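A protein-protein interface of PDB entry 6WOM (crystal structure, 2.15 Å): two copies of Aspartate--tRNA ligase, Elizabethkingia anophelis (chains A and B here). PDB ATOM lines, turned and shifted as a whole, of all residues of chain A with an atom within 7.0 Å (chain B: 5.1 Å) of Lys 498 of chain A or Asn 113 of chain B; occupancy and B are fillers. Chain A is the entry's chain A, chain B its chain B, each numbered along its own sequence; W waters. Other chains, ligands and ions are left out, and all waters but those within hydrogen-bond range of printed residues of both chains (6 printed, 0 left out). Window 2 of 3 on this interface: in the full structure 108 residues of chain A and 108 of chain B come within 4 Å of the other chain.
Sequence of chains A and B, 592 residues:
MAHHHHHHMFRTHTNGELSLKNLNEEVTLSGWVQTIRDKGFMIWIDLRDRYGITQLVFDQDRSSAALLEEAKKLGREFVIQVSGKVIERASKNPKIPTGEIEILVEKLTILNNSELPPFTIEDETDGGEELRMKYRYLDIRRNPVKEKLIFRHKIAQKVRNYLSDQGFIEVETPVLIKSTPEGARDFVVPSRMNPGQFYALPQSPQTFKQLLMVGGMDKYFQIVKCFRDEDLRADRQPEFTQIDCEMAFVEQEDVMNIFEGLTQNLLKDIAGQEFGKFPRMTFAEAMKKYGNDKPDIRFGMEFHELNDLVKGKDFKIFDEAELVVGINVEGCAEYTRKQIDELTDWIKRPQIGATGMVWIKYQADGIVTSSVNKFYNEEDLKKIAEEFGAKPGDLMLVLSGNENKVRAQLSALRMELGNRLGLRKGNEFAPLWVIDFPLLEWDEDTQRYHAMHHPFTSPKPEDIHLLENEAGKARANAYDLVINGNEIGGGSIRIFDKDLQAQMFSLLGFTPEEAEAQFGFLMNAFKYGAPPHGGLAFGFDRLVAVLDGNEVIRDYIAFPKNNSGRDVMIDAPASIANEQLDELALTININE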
ATOM      1  N   ILE A 495       9.044  -1.012  -5.983  1.00  0.00           N
ATOM      2  CA  ILE A 495       8.045  -0.080  -6.498  1.00  0.00           C
ATOM      3  C   ILE A 495       6.727  -0.330  -5.782  1.00  0.00           C
ATOM      4  O   ILE A 495       6.314  -1.481  -5.610  1.00  0.00           O
ATOM      5  CB  ILE A 495       7.890  -0.255  -8.021  1.00  0.00           C
ATOM      6  CG1 ILE A 495       9.172   0.152  -8.747  1.00  0.00           C
ATOM      7  CG2 ILE A 495       6.679   0.495  -8.560  1.00  0.00           C
ATOM      8  CD1 ILE A 495       9.199  -0.290 -10.193  1.00  0.00           C
ATOM      9  N   PHE A 496       6.066   0.745  -5.349  1.00  0.00           N
ATOM     10  CA  PHE A 496       4.706   0.643  -4.826  1.00  0.00           C
ATOM     11  C   PHE A 496       3.692   1.414  -5.659  1.00  0.00           C
ATOM     12  O   PHE A 496       2.487   1.310  -5.398  1.00  0.00           O
ATOM     13  CB  PHE A 496       4.639   1.151  -3.375  1.00  0.00           C
ATOM     14  CG  PHE A 496       5.009   2.606  -3.208  1.00  0.00           C
ATOM     15  CD1 PHE A 496       4.031   3.600  -3.265  1.00  0.00           C
ATOM     16  CD2 PHE A 496       6.336   2.977  -2.963  1.00  0.00           C
ATOM     17  CE1 PHE A 496       4.375   4.958  -3.107  1.00  0.00           C
ATOM     18  CE2 PHE A 496       6.697   4.306  -2.789  1.00  0.00           C
ATOM     19  CZ  PHE A 496       5.714   5.315  -2.873  1.00  0.00           C
ATOM     20  N   ASP A 497       4.153   2.166  -6.650  1.00  0.00           N
ATOM     21  CA  ASP A 497       3.313   2.975  -7.522  1.00  0.00           C
ATOM     22  C   ASP A 497       2.958   2.185  -8.775  1.00  0.00           C
ATOM     23  O   ASP A 497       3.833   1.866  -9.589  1.00  0.00           O
ATOM     24  CB  ASP A 497       4.030   4.272  -7.904  1.00  0.00           C
ATOM     25  CG  ASP A 497       3.176   5.154  -8.812  1.00  0.00           C
ATOM     26  OD1 ASP A 497       2.542   6.073  -8.286  1.00  0.00           O
ATOM     27  OD2 ASP A 497       3.106   4.899 -10.032  1.00  0.00           O
ATOM     28  N   LYS A 498       1.670   1.911  -8.935  1.00  0.00           N
ATOM     29  CA  LYS A 498       1.193   1.046 -10.001  1.00  0.00           C
ATOM     30  C   LYS A 498       1.588   1.586 -11.376  1.00  0.00           C
ATOM     31  O   LYS A 498       1.986   0.821 -12.264  1.00  0.00           O
ATOM     32  CB  LYS A 498      -0.336   0.939  -9.842  1.00  0.00           C
ATOM     33  CG  LYS A 498      -1.123   0.172 -10.868  1.00  0.00           C
ATOM     34  CD  LYS A 498      -2.515  -0.200 -10.311  1.00  0.00           C
ATOM     35  CE  LYS A 498      -3.370   1.028  -9.966  1.00  0.00           C
ATOM     36  NZ  LYS A 498      -3.224   1.499  -8.551  1.00  0.00           N
ATOM     37  N   ASP A 499       1.585   2.908 -11.537  1.00  0.00           N
ATOM     38  CA  ASP A 499       1.960   3.505 -12.817  1.00  0.00           C
ATOM     39  C   ASP A 499       3.451   3.392 -13.086  1.00  0.00           C
ATOM     40  O   ASP A 499       3.863   3.164 -14.235  1.00  0.00           O
ATOM     41  CB  ASP A 499       1.532   4.967 -12.862  1.00  0.00           C
ATOM     42  CG  ASP A 499       0.031   5.127 -12.836  1.00  0.00           C
ATOM     43  OD1 ASP A 499      -0.666   4.128 -13.097  1.00  0.00           O
ATOM     44  OD2 ASP A 499      -0.450   6.248 -12.566  1.00  0.00           O
ATOM     45  N   LEU A 500       4.285   3.589 -12.060  1.00  0.00           N
ATOM     46  CA  LEU A 500       5.722   3.412 -12.269  1.00  0.00           C
ATOM     47  C   LEU A 500       6.032   1.979 -12.682  1.00  0.00           C
ATOM     48  O   LEU A 500       6.853   1.744 -13.575  1.00  0.00           O
ATOM     49  CB  LEU A 500       6.505   3.793 -10.999  1.00  0.00           C
ATOM     50  CG  LEU A 500       8.035   3.618 -11.008  1.00  0.00           C
ATOM     51  CD1 LEU A 500       8.635   4.365 -12.166  1.00  0.00           C
ATOM     52  CD2 LEU A 500       8.705   4.057  -9.675  1.00  0.00           C
ATOM     53  N   GLN A 501       5.363   1.007 -12.056  1.00  0.00           N
ATOM     54  CA  GLN A 501       5.616  -0.396 -12.380  1.00  0.00           C
ATOM     55  C   GLN A 501       5.282  -0.700 -13.840  1.00  0.00           C
ATOM     56  O   GLN A 501       6.061  -1.358 -14.542  1.00  0.00           O
ATOM     57  CB  GLN A 501       4.802  -1.296 -11.456  1.00  0.00           C
ATOM     58  CG  GLN A 501       5.158  -2.761 -11.609  1.00  0.00           C
ATOM     59  CD  GLN A 501       6.603  -3.004 -11.262  1.00  0.00           C
ATOM     60  OE1 GLN A 501       6.981  -2.965 -10.091  1.00  0.00           O
ATOM     61  NE2 GLN A 501       7.442  -3.197 -12.283  1.00  0.00           N
ATOM     62  N   ALA A 502       4.127  -0.214 -14.319  1.00  0.00           N
ATOM     63  CA  ALA A 502       3.746  -0.445 -15.714  1.00  0.00           C
ATOM     64  C   ALA A 502       4.750   0.192 -16.659  1.00  0.00           C
ATOM     65  O   ALA A 502       5.128  -0.398 -17.676  1.00  0.00           O
ATOM     66  CB  ALA A 502       2.347   0.125 -15.987  1.00  0.00           C
ATOM     67  N   GLN A 503       5.231   1.378 -16.307  1.00  0.00           N
ATOM     68  CA  GLN A 503       6.243   2.043 -17.121  1.00  0.00           C
ATOM     69  C   GLN A 503       7.537   1.244 -17.166  1.00  0.00           C
ATOM     70  O   GLN A 503       8.204   1.180 -18.206  1.00  0.00           O
ATOM     71  CB  GLN A 503       6.503   3.433 -16.553  1.00  0.00           C
ATOM     72  CG  GLN A 503       7.696   4.113 -17.125  1.00  0.00           C
ATOM     73  CD  GLN A 503       7.738   5.550 -16.694  1.00  0.00           C
ATOM     74  OE1 GLN A 503       7.270   5.885 -15.605  1.00  0.00           O
ATOM     75  NE2 GLN A 503       8.228   6.426 -17.574  1.00  0.00           N
ATOM     76  N   MET A 523       1.161  -8.458  -8.354  1.00  0.00           N
ATOM     77  CA  MET A 523       0.573  -7.191  -8.783  1.00  0.00           C
ATOM     78  C   MET A 523      -0.880  -7.101  -8.366  1.00  0.00           C
ATOM     79  O   MET A 523      -1.337  -6.045  -7.902  1.00  0.00           O
ATOM     80  CB  MET A 523       0.709  -7.000 -10.299  1.00  0.00           C
ATOM     81  CG  MET A 523       2.137  -6.718 -10.744  1.00  0.00           C
ATOM     82  SD  MET A 523       2.268  -6.315 -12.506  1.00  0.00           S
ATOM     83  CE  MET A 523       1.470  -7.720 -13.268  1.00  0.00           C
ATOM     84  N   PHE A 526      -0.943  -6.419  -4.629  1.00  0.00           N
ATOM     85  CA  PHE A 526      -0.522  -5.064  -4.277  1.00  0.00           C
ATOM     86  C   PHE A 526      -1.669  -4.057  -4.366  1.00  0.00           C
ATOM     87  O   PHE A 526      -1.658  -3.047  -3.651  1.00  0.00           O
ATOM     88  CB  PHE A 526       0.631  -4.629  -5.192  1.00  0.00           C
ATOM     89  CG  PHE A 526       1.944  -5.346  -4.930  1.00  0.00           C
ATOM     90  CD1 PHE A 526       2.115  -6.163  -3.806  1.00  0.00           C
ATOM     91  CD2 PHE A 526       2.999  -5.231  -5.838  1.00  0.00           C
ATOM     92  CE1 PHE A 526       3.295  -6.819  -3.588  1.00  0.00           C
ATOM     93  CE2 PHE A 526       4.198  -5.878  -5.618  1.00  0.00           C
ATOM     94  CZ  PHE A 526       4.352  -6.673  -4.492  1.00  0.00           C
ATOM     95  N   LYS A 527      -2.669  -4.315  -5.222  1.00  0.00           N
ATOM     96  CA  LYS A 527      -3.764  -3.370  -5.404  1.00  0.00           C
ATOM     97  C   LYS A 527      -4.644  -3.228  -4.168  1.00  0.00           C
ATOM     98  O   LYS A 527      -5.404  -2.257  -4.086  1.00  0.00           O
ATOM     99  CB  LYS A 527      -4.613  -3.768  -6.618  1.00  0.00           C
ATOM    100  CG  LYS A 527      -5.765  -4.699  -6.253  1.00  0.00           C
ATOM    101  CD  LYS A 527      -6.296  -5.480  -7.458  1.00  0.00           C
ATOM    102  CE  LYS A 527      -7.662  -6.075  -7.116  1.00  0.00           C
ATOM    103  NZ  LYS A 527      -8.059  -7.175  -8.036  1.00  0.00           N
ATOM    104  N   TYR A 528      -4.573  -4.164  -3.215  1.00  0.00           N
ATOM    105  CA  TYR A 528      -5.301  -4.068  -1.959  1.00  0.00           C
ATOM    106  C   TYR A 528      -4.527  -3.317  -0.873  1.00  0.00           C
ATOM    107  O   TYR A 528      -4.970  -3.280   0.281  1.00  0.00           O
ATOM    108  CB  TYR A 528      -5.671  -5.457  -1.446  1.00  0.00           C
ATOM    109  CG  TYR A 528      -6.691  -6.161  -2.280  1.00  0.00           C
ATOM    110  CD1 TYR A 528      -8.026  -5.781  -2.244  1.00  0.00           C
ATOM    111  CD2 TYR A 528      -6.327  -7.210  -3.105  1.00  0.00           C
ATOM    112  CE1 TYR A 528      -8.972  -6.433  -3.009  1.00  0.00           C
ATOM    113  CE2 TYR A 528      -7.253  -7.854  -3.882  1.00  0.00           C
ATOM    114  CZ  TYR A 528      -8.574  -7.475  -3.831  1.00  0.00           C
ATOM    115  OH  TYR A 528      -9.489  -8.151  -4.610  1.00  0.00           O
ATOM    116  N   GLY A 529      -3.399  -2.696  -1.215  1.00  0.00           N
ATOM    117  CA  GLY A 529      -2.733  -1.821  -0.277  1.00  0.00           C
ATOM    118  C   GLY A 529      -1.293  -2.161   0.049  1.00  0.00           C
ATOM    119  O   GLY A 529      -0.897  -2.109   1.218  1.00  0.00           O
ATOM    120  N   PHE B  78      -6.834   2.479   2.085  1.00  0.00           N
ATOM    121  CA  PHE B  78      -5.855   3.313   1.372  1.00  0.00           C
ATOM    122  C   PHE B  78      -4.575   3.400   2.200  1.00  0.00           C
ATOM    123  O   PHE B  78      -4.628   3.456   3.432  1.00  0.00           O
ATOM    124  CB  PHE B  78      -6.404   4.744   1.146  1.00  0.00           C
ATOM    125  CG  PHE B  78      -7.221   4.929  -0.140  1.00  0.00           C
ATOM    126  CD1 PHE B  78      -8.145   3.975  -0.556  1.00  0.00           C
ATOM    127  CD2 PHE B  78      -7.091   6.096  -0.897  1.00  0.00           C
ATOM    128  CE1 PHE B  78      -8.914   4.172  -1.730  1.00  0.00           C
ATOM    129  CE2 PHE B  78      -7.845   6.295  -2.050  1.00  0.00           C
ATOM    130  CZ  PHE B  78      -8.763   5.328  -2.465  1.00  0.00           C
ATOM    131  N   ILE B 110      -1.586  10.324  -0.930  1.00  0.00           N
ATOM    132  CA  ILE B 110      -2.096   8.974  -1.143  1.00  0.00           C
ATOM    133  C   ILE B 110      -0.958   8.146  -1.734  1.00  0.00           C
ATOM    134  O   ILE B 110      -0.527   8.388  -2.861  1.00  0.00           O
ATOM    135  CB  ILE B 110      -3.322   8.977  -2.061  1.00  0.00           C
ATOM    136  CG1 ILE B 110      -4.447   9.806  -1.436  1.00  0.00           C
ATOM    137  CG2 ILE B 110      -3.790   7.555  -2.347  1.00  0.00           C
ATOM    138  CD1 ILE B 110      -5.709   9.893  -2.313  1.00  0.00           C
ATOM    139  N   LEU B 111      -0.476   7.157  -0.977  1.00  0.00           N
ATOM    140  CA  LEU B 111       0.596   6.306  -1.469  1.00  0.00           C
ATOM    141  C   LEU B 111       0.055   5.140  -2.286  1.00  0.00           C
ATOM    142  O   LEU B 111       0.680   4.734  -3.268  1.00  0.00           O
ATOM    143  CB  LEU B 111       1.432   5.784  -0.292  1.00  0.00           C
ATOM    144  CG  LEU B 111       2.113   6.834   0.591  1.00  0.00           C
ATOM    145  CD1 LEU B 111       2.713   6.167   1.840  1.00  0.00           C
ATOM    146  CD2 LEU B 111       3.164   7.637  -0.190  1.00  0.00           C
ATOM    147  N   ASN B 112      -1.124   4.638  -1.930  1.00  0.00           N
ATOM    148  CA  ASN B 112      -1.779   3.561  -2.666  1.00  0.00           C
ATOM    149  C   ASN B 112      -3.288   3.719  -2.514  1.00  0.00           C
ATOM    150  O   ASN B 112      -3.811   3.604  -1.400  1.00  0.00           O
ATOM    151  CB  ASN B 112      -1.328   2.185  -2.142  1.00  0.00           C
ATOM    152  CG  ASN B 112      -1.716   1.043  -3.073  1.00  0.00           C
ATOM    153  OD1 ASN B 112      -2.711   1.130  -3.812  1.00  0.00           O
ATOM    154  ND2 ASN B 112      -0.935  -0.043  -3.035  1.00  0.00           N
ATOM    155  N   ASN B 113      -3.992   3.959  -3.622  1.00  0.00           N
ATOM    156  CA  ASN B 113      -5.456   4.048  -3.590  1.00  0.00           C
ATOM    157  C   ASN B 113      -6.034   2.636  -3.697  1.00  0.00           C
ATOM    158  O   ASN B 113      -6.589   2.220  -4.718  1.00  0.00           O
ATOM    159  CB  ASN B 113      -5.970   4.970  -4.697  1.00  0.00           C
ATOM    160  CG  ASN B 113      -5.469   4.567  -6.058  1.00  0.00           C
ATOM    161  OD1 ASN B 113      -4.327   4.115  -6.186  1.00  0.00           O
ATOM    162  ND2 ASN B 113      -6.308   4.708  -7.083  1.00  0.00           N
ATOM    163  N   SER B 114      -5.916   1.915  -2.579  1.00  0.00           N
ATOM    164  CA  SER B 114      -6.244   0.502  -2.511  1.00  0.00           C
ATOM    165  C   SER B 114      -7.694   0.250  -2.906  1.00  0.00           C
ATOM    166  O   SER B 114      -8.590   1.049  -2.608  1.00  0.00           O
ATOM    167  CB  SER B 114      -6.045  -0.023  -1.080  1.00  0.00           C
ATOM    168  OG  SER B 114      -4.925   0.580  -0.479  1.00  0.00           O
ATOM    169  N   GLU B 115      -7.927  -0.900  -3.542  1.00  0.00           N
ATOM    170  CA  GLU B 115      -9.283  -1.414  -3.638  1.00  0.00           C
ATOM    171  C   GLU B 115      -9.789  -1.755  -2.245  1.00  0.00           C
ATOM    172  O   GLU B 115      -9.018  -1.998  -1.311  1.00  0.00           O
ATOM    173  CB  GLU B 115      -9.346  -2.667  -4.514  1.00  0.00           C
ATOM    174  CG  GLU B 115      -8.635  -2.542  -5.843  1.00  0.00           C
ATOM    175  CD  GLU B 115      -9.526  -2.019  -6.957  1.00  0.00           C
ATOM    176  OE1 GLU B 115     -10.484  -1.260  -6.656  1.00  0.00           O
ATOM    177  OE2 GLU B 115      -9.260  -2.369  -8.137  1.00  0.00           O
HETATM  178  O   HOH W   1      -6.093   3.054  -9.614  1.00  0.00           O
HETATM  179  O   HOH W   2      -2.782   0.261  -6.403  1.00  0.00           O
HETATM  180  O   HOH W   3      -0.061   2.094  -5.739  1.00  0.00           O
HETATM  181  O   HOH W   4       1.849   5.992  -5.600  1.00  0.00           O
HETATM  182  O   HOH W   5      -7.954  -3.694   0.778  1.00  0.00           O
HETATM  183  O   HOH W   6      -5.863  -0.116  -6.770  1.00  0.00           O
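O of Phe 526 of chain A sits at hydrogen-bond distance from ND2 of Asn 112 of chain B. The backbone NH (N) of Glu 115 of chain B lies within hydrogen-bond range of the backbone carbonyl oxygen (O) of Lys 527 of chain A, 2.9 Å away.
O of Asn 112 of chain B is in hydrogen-bond range of OG of Ser 114 of chain B, at 3.4 Å.
Among the printed residues, merely in contact across the chains: Gly 529 of chain A with Ser 114 of chain B (3.3 Å), Lys 527 of chain A with Ser 114 of chain B (3.3 Å), Phe 496 of chain A with Leu 111 of chain B (3.5 Å), Tyr 528 of chain A with Ser 114 of chain B (3.6 Å), Lys 498 of chain A with Asn 113 of chain B (3.7 Å) and Gly 529 of chain A with Asn 112 of chain B (3.7 Å).
Lys 498 of chain A touches just one residue of chain B: Asn 113. Of the printed residues of chain A, Asn 113 of chain B touches Lys 498 (3.7 Å). Of the printed residues of chain B, Lys 527 of chain A touches Ser 114 (3.3 Å) and Glu 115 (2.9 Å). Of the printed residues of chain B, Phe 526 of chain A touches Asn 112 (3.2 Å). Printed residues of chain A within 4 Å of Asn 112 of chain B: Phe 526 and Gly 529. The nearest printed residue of chain A that does not touch Leu 111 of chain B is Asp 497 of chain A (5.3 Å).
Printed residues of chain B that touch a printed residue of chain A: Leu 111, Asn 112, Asn 113, Ser 114 and Glu 115.
No position is printed for both chains. Of the 8 pairs that touch across the chains among the printed residues, none has its exchanged pair printed and touching as well.
Water W2 lies within hydrogen-bond range of NZ of Lys 498 of chain A (2.5 Å) and OD1 of Asn 112 of chain B (2.7 Å). Water W3 bridges O of Phe 496 of chain A and OD1 of Asn 112 of chain B. Water W4 lies within hydrogen-bond range of OD1 of Asp 497 of chain A and O of Leu 111 of chain B. Water W5 lies within hydrogen-bond range of the backbone carbonyl oxygen (O) of Glu 115 of chain B (2.9 Å) and the backbone carbonyl oxygen (O) of Tyr 528 of chain A (3.1 Å). Water W1 bridges the side-chain amide nitrogen of Asn 113 of chain B and the side-chain amino group of Lys 498 of chain A. Water W6 bridges O of Asn 113 of chain B and O of Lys 527 of chain A.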
